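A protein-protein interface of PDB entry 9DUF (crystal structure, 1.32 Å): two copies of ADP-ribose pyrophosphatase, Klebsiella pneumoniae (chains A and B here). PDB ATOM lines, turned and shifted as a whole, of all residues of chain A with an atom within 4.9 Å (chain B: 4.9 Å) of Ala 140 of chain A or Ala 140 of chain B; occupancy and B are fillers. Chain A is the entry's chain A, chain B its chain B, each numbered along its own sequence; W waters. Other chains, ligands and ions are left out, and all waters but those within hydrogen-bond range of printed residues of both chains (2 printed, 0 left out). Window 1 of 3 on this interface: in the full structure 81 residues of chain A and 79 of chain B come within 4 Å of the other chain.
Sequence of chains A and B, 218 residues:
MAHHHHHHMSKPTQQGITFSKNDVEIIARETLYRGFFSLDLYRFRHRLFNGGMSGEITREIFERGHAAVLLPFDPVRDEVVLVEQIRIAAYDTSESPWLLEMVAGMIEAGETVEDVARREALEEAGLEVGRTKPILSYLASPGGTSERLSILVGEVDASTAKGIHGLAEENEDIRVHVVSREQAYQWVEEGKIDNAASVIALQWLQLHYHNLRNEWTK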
ATOM      1  N   TYR A 138      -4.160  16.249  -0.423  1.00  0.00           N
ATOM      2  CA  TYR A 138      -2.829  16.658   0.012  1.00  0.00           C
ATOM      3  C   TYR A 138      -1.766  15.620  -0.323  1.00  0.00           C
ATOM      4  O   TYR A 138      -2.044  14.425  -0.440  1.00  0.00           O
ATOM      5  CB  TYR A 138      -2.812  16.970   1.530  1.00  0.00           C
ATOM      6  CG  TYR A 138      -2.961  15.756   2.418  1.00  0.00           C
ATOM      7  CD1 TYR A 138      -4.217  15.250   2.725  1.00  0.00           C
ATOM      8  CD2 TYR A 138      -1.849  15.110   2.931  1.00  0.00           C
ATOM      9  CE1 TYR A 138      -4.356  14.123   3.509  1.00  0.00           C
ATOM     10  CE2 TYR A 138      -1.982  13.992   3.722  1.00  0.00           C
ATOM     11  CZ  TYR A 138      -3.244  13.499   4.004  1.00  0.00           C
ATOM     12  OH  TYR A 138      -3.403  12.363   4.767  1.00  0.00           O
ATOM     13  N   LEU A 139      -0.537  16.110  -0.480  1.00  0.00           N
ATOM     14  CA  LEU A 139       0.646  15.273  -0.605  1.00  0.00           C
ATOM     15  C   LEU A 139       1.171  14.974   0.795  1.00  0.00           C
ATOM     16  O   LEU A 139       1.465  15.890   1.568  1.00  0.00           O
ATOM     17  CB  LEU A 139       1.698  16.005  -1.431  1.00  0.00           C
ATOM     18  CG  LEU A 139       1.295  16.227  -2.884  1.00  0.00           C
ATOM     19  CD1 LEU A 139       2.083  17.385  -3.488  1.00  0.00           C
ATOM     20  CD2 LEU A 139       1.494  14.966  -3.735  1.00  0.00           C
ATOM     21  N   ALA A 140       1.295  13.689   1.109  1.00  0.00           N
ATOM     22  CA  ALA A 140       1.654  13.286   2.465  1.00  0.00           C
ATOM     23  C   ALA A 140       3.022  13.795   2.884  1.00  0.00           C
ATOM     24  O   ALA A 140       3.199  14.225   4.031  1.00  0.00           O
ATOM     25  CB  ALA A 140       1.628  11.767   2.579  1.00  0.00           C
ATOM     26  N   SER A 141       4.002  13.702   1.999  1.00  0.00           N
ATOM     27  CA  SER A 141       5.389  14.032   2.322  1.00  0.00           C
ATOM     28  C   SER A 141       6.184  14.085   1.021  1.00  0.00           C
ATOM     29  O   SER A 141       6.949  13.161   0.701  1.00  0.00           O
ATOM     30  CB  SER A 141       5.980  13.015   3.278  1.00  0.00           C
ATOM     31  OG  SER A 141       7.265  13.427   3.662  1.00  0.00           O
ATOM     32  N   PRO A 142       6.026  15.162   0.250  1.00  0.00           N
ATOM     33  CA  PRO A 142       6.470  15.144  -1.148  1.00  0.00           C
ATOM     34  C   PRO A 142       7.964  15.213  -1.371  1.00  0.00           C
ATOM     35  O   PRO A 142       8.368  15.130  -2.528  1.00  0.00           O
ATOM     36  CB  PRO A 142       5.721  16.321  -1.764  1.00  0.00           C
ATOM     37  CG  PRO A 142       5.467  17.254  -0.615  1.00  0.00           C
ATOM     38  CD  PRO A 142       5.187  16.342   0.546  1.00  0.00           C
ATOM     39  N   THR A 145       7.951  10.850  -1.059  1.00  0.00           N
ATOM     40  CA  THR A 145       6.915   9.949  -1.535  1.00  0.00           C
ATOM     41  C   THR A 145       5.967  10.720  -2.445  1.00  0.00           C
ATOM     42  O   THR A 145       5.709  11.904  -2.231  1.00  0.00           O
ATOM     43  CB  THR A 145       6.136   9.254  -0.378  1.00  0.00           C
ATOM     44  OG1 THR A 145       5.134   8.377  -0.921  1.00  0.00           O
ATOM     45  CG2 THR A 145       5.442  10.236   0.526  1.00  0.00           C
ATOM     46  N   GLU A 147       2.842  10.015  -2.669  1.00  0.00           N
ATOM     47  CA  GLU A 147       1.489   9.719  -2.226  1.00  0.00           C
ATOM     48  C   GLU A 147       0.651  10.981  -2.063  1.00  0.00           C
ATOM     49  O   GLU A 147       1.019  11.911  -1.324  1.00  0.00           O
ATOM     50  CB  GLU A 147       1.511   8.970  -0.893  1.00  0.00           C
ATOM     51  CG  GLU A 147       0.132   8.462  -0.528  1.00  0.00           C
ATOM     52  CD  GLU A 147       0.053   7.819   0.825  1.00  0.00           C
ATOM     53  OE1 GLU A 147       0.915   8.087   1.675  1.00  0.00           O
ATOM     54  OE2 GLU A 147      -0.923   7.082   1.038  1.00  0.00           O
ATOM     55  N   LEU A 149      -3.404  11.940  -0.948  1.00  0.00           N
ATOM     56  CA  LEU A 149      -4.594  11.447  -0.273  1.00  0.00           C
ATOM     57  C   LEU A 149      -5.684  12.492  -0.433  1.00  0.00           C
ATOM     58  O   LEU A 149      -5.463  13.661  -0.131  1.00  0.00           O
ATOM     59  CB  LEU A 149      -4.339  11.193   1.217  1.00  0.00           C
ATOM     60  CG  LEU A 149      -3.254  10.145   1.508  1.00  0.00           C
ATOM     61  CD1 LEU A 149      -1.878  10.788   1.648  1.00  0.00           C
ATOM     62  CD2 LEU A 149      -3.592   9.343   2.738  1.00  0.00           C
ATOM     63  N   ALA A 196      -1.498  12.296   9.804  1.00  0.00           N
ATOM     64  CA  ALA A 196      -1.821  13.450   8.976  1.00  0.00           C
ATOM     65  C   ALA A 196      -3.269  13.471   8.505  1.00  0.00           C
ATOM     66  O   ALA A 196      -3.917  14.511   8.535  1.00  0.00           O
ATOM     67  CB  ALA A 196      -0.899  13.508   7.763  1.00  0.00           C
ATOM     68  N   TYR B 138       3.221  14.923  13.846  1.00  0.00           N
ATOM     69  CA  TYR B 138       2.342  14.006  13.135  1.00  0.00           C
ATOM     70  C   TYR B 138       3.118  12.975  12.330  1.00  0.00           C
ATOM     71  O   TYR B 138       4.247  13.210  11.895  1.00  0.00           O
ATOM     72  CB  TYR B 138       1.349  14.761  12.203  1.00  0.00           C
ATOM     73  CG  TYR B 138       2.008  15.396  10.999  1.00  0.00           C
ATOM     74  CD1 TYR B 138       2.592  16.653  11.085  1.00  0.00           C
ATOM     75  CD2 TYR B 138       2.022  14.762   9.759  1.00  0.00           C
ATOM     76  CE1 TYR B 138       3.220  17.221  10.004  1.00  0.00           C
ATOM     77  CE2 TYR B 138       2.637  15.327   8.665  1.00  0.00           C
ATOM     78  CZ  TYR B 138       3.234  16.561   8.793  1.00  0.00           C
ATOM     79  OH  TYR B 138       3.869  17.164   7.741  1.00  0.00           O
ATOM     80  N   LEU B 139       2.479  11.832  12.130  1.00  0.00           N
ATOM     81  CA  LEU B 139       2.941  10.792  11.219  1.00  0.00           C
ATOM     82  C   LEU B 139       2.417  11.087   9.819  1.00  0.00           C
ATOM     83  O   LEU B 139       1.209  11.223   9.613  1.00  0.00           O
ATOM     84  CB  LEU B 139       2.454   9.435  11.718  1.00  0.00           C
ATOM     85  CG  LEU B 139       3.007   9.022  13.075  1.00  0.00           C
ATOM     86  CD1 LEU B 139       2.114   7.987  13.703  1.00  0.00           C
ATOM     87  CD2 LEU B 139       4.419   8.474  12.874  1.00  0.00           C
ATOM     88  N   ALA B 140       3.341  11.250   8.867  1.00  0.00           N
ATOM     89  CA  ALA B 140       2.959  11.635   7.513  1.00  0.00           C
ATOM     90  C   ALA B 140       1.994  10.651   6.864  1.00  0.00           C
ATOM     91  O   ALA B 140       1.056  11.066   6.179  1.00  0.00           O
ATOM     92  CB  ALA B 140       4.213  11.787   6.653  1.00  0.00           C
ATOM     93  N   SER B 141       2.243   9.347   7.004  1.00  0.00           N
ATOM     94  CA  SER B 141       1.446   8.340   6.303  1.00  0.00           C
ATOM     95  C   SER B 141       1.789   6.982   6.900  1.00  0.00           C
ATOM     96  O   SER B 141       2.544   6.199   6.305  1.00  0.00           O
ATOM     97  CB  SER B 141       1.720   8.338   4.809  1.00  0.00           C
ATOM     98  OG  SER B 141       0.852   7.435   4.150  1.00  0.00           O
ATOM     99  N   PRO B 142       1.288   6.687   8.099  1.00  0.00           N
ATOM    100  CA  PRO B 142       1.855   5.589   8.888  1.00  0.00           C
ATOM    101  C   PRO B 142       1.497   4.201   8.406  1.00  0.00           C
ATOM    102  O   PRO B 142       1.998   3.248   8.989  1.00  0.00           O
ATOM    103  CB  PRO B 142       1.324   5.867  10.293  1.00  0.00           C
ATOM    104  CG  PRO B 142       0.060   6.646  10.063  1.00  0.00           C
ATOM    105  CD  PRO B 142       0.331   7.498   8.873  1.00  0.00           C
ATOM    106  N   THR B 145       5.099   4.500   5.941  1.00  0.00           N
ATOM    107  CA  THR B 145       6.341   5.169   6.294  1.00  0.00           C
ATOM    108  C   THR B 145       6.329   5.487   7.778  1.00  0.00           C
ATOM    109  O   THR B 145       5.277   5.768   8.356  1.00  0.00           O
ATOM    110  CB  THR B 145       6.592   6.441   5.438  1.00  0.00           C
ATOM    111  OG1 THR B 145       7.844   7.034   5.812  1.00  0.00           O
ATOM    112  CG2 THR B 145       5.510   7.477   5.590  1.00  0.00           C
ATOM    113  N   GLU B 147       7.826   8.063   8.991  1.00  0.00           N
ATOM    114  CA  GLU B 147       8.198   9.458   9.132  1.00  0.00           C
ATOM    115  C   GLU B 147       7.258  10.223  10.039  1.00  0.00           C
ATOM    116  O   GLU B 147       6.039  10.251   9.828  1.00  0.00           O
ATOM    117  CB  GLU B 147       8.246  10.147   7.766  1.00  0.00           C
ATOM    118  CG  GLU B 147       8.826  11.556   7.874  1.00  0.00           C
ATOM    119  CD  GLU B 147       8.736  12.352   6.603  1.00  0.00           C
ATOM    120  OE1 GLU B 147       7.891  12.054   5.738  1.00  0.00           O
ATOM    121  OE2 GLU B 147       9.513  13.318   6.503  1.00  0.00           O
ATOM    122  N   LEU B 149       6.902  14.225  11.645  1.00  0.00           N
ATOM    123  CA  LEU B 149       7.288  15.612  11.426  1.00  0.00           C
ATOM    124  C   LEU B 149       6.754  16.418  12.599  1.00  0.00           C
ATOM    125  O   LEU B 149       5.561  16.349  12.915  1.00  0.00           O
ATOM    126  CB  LEU B 149       6.727  16.160  10.106  1.00  0.00           C
ATOM    127  CG  LEU B 149       7.198  15.427   8.849  1.00  0.00           C
ATOM    128  CD1 LEU B 149       6.274  14.323   8.456  1.00  0.00           C
ATOM    129  CD2 LEU B 149       7.389  16.388   7.667  1.00  0.00           C
ATOM    130  N   ALA B 196       1.059  18.195   3.297  1.00  0.00           N
ATOM    131  CA  ALA B 196       0.560  17.977   4.652  1.00  0.00           C
ATOM    132  C   ALA B 196       1.120  18.966   5.664  1.00  0.00           C
ATOM    133  O   ALA B 196       0.371  19.512   6.483  1.00  0.00           O
ATOM    134  CB  ALA B 196       0.831  16.543   5.104  1.00  0.00           C
HETATM  135  O   HOH W   1       4.634  15.765   5.518  1.00  0.00           O
HETATM  136  O   HOH W   2      -1.467  10.630   5.432  1.00  0.00           O
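Of the printed residues of chain B, Leu 139 of chain A touches Ala 196.
Of chain B, only Ala 140 and Ala 196 come within 4 Å of Ala 140 of chain A.
Printed residues of chain B within 4 Å of Ser 141 of chain A: Glu 147 (2.6 Å).
Thr 145 of chain A touches none of the printed residues of chain B.
Of the printed residues of chain B, Ala 196 of chain A touches Tyr 138 (3.8 Å), Leu 139 (2.9 Å) and Ala 140 (3.5 Å).
Of the printed residues of chain A, Tyr 138 of chain B touches Ala 196 (3.8 Å).
Printed residues of chain A within 4 Å of Ala 140 of chain B: Ala 140 (3.7 Å) and Ala 196 (3.5 Å).
Pro 142 of chain B touches none of the printed residues of chain A.
Of the printed residues of chain A, Ala 196 of chain B touches Tyr 138 (3.7 Å), Leu 139 (2.9 Å) and Ala 140 (3.5 Å).
The nearest printed residue of chain A that does not touch Ala 140 of chain B is Ser 141 of chain A (4.003 Å).
CD2 of Tyr 138 of chain A touches CB of Ala 196 of chain B, 3.7 Å away.
Ala 140 of chain A touches Ala 140 of chain B (CB to O, 3.7 Å).
Ala 140 of chain A touches Ala 196 of chain B (O to CB, 3.5 Å).
CB of Ala 196 of chain A touches CD2 of Tyr 138 of chain B, 3.8 Å away.
CB of Ala 196 of chain A touches O of Ala 140 of chain B (3.5 Å).
The backbone NH of Ala 196 of chain B lies within hydrogen-bond range of the backbone carbonyl oxygen of Leu 139 of chain A.
The side-chain carboxylate (OE1) of Glu 147 of chain B is in hydrogen-bond range of the side-chain hydroxyl (OG) of Ser 141 of chain A (2.6 Å).
OG of Ser 141 of chain B sits at hydrogen-bond distance from OE1 of Glu 147 of chain A, 2.6 Å away.
The backbone NH (N) of Ala 196 of chain A is in hydrogen-bond range of the backbone carbonyl oxygen (O) of Leu 139 of chain B (2.9 Å).
The backbone NH (N) of Leu 149 of chain A lies within hydrogen-bond range of the backbone carbonyl oxygen (O) of Tyr 138 of chain A (2.9 Å).
O of Glu 147 of chain A sits at hydrogen-bond distance from N of Ala 140 of chain A (3.0 Å).
The side-chain hydroxyl (OG1) of Thr 145 of chain A sits close to the backbone NH (N) of Glu 147 of chain A (3.3 Å).
N of Leu 149 of chain B is in hydrogen-bond range of O of Tyr 138 of chain B, 2.9 Å away.
The backbone NH (N) of Ala 140 of chain B lies within hydrogen-bond range of the backbone carbonyl oxygen (O) of Glu 147 of chain B (3.0 Å).
The side-chain hydroxyl (OG1) of Thr 145 of chain B sits close to the backbone NH (N) of Glu 147 of chain B, at 3.3 Å.
Water W1 bridges the backbone carbonyl oxygen of Ala 140 of chain A (2.6 Å) and the side-chain hydroxyl of Tyr 138 of chain B (2.7 Å).
Water W2 bridges the backbone carbonyl oxygen of Ala 140 of chain B (2.7 Å) and the side-chain hydroxyl of Tyr 138 of chain A (2.7 Å).
Tyr 138 of chain A touches Ala 196 of chain B, and with the chains exchanged Ala 196 of chain A touches Tyr 138 of chain B.
Leu 139 of chain A touches Ala 196 of chain B, and with the chains exchanged Ala 196 of chain A touches Leu 139 of chain B.
Ala 140 of chain A touches its own counterpart, Ala 140 of chain B.
Ala 140 of chain A touches Ala 196 of chain B, and with the chains exchanged Ala 196 of chain A touches Ala 140 of chain B.
9 positions are printed for both chains.
Of the 9 pairs that touch across the chains among the printed residues, 9 have their exchanged pair printed and touching as well.
Among the printed residues, 9 pairs touch across the chains.
Among the printed residues, no Asp or Glu carboxylate lies within 4 Å of a Lys or Arg side-chain nitrogen of the other chain.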
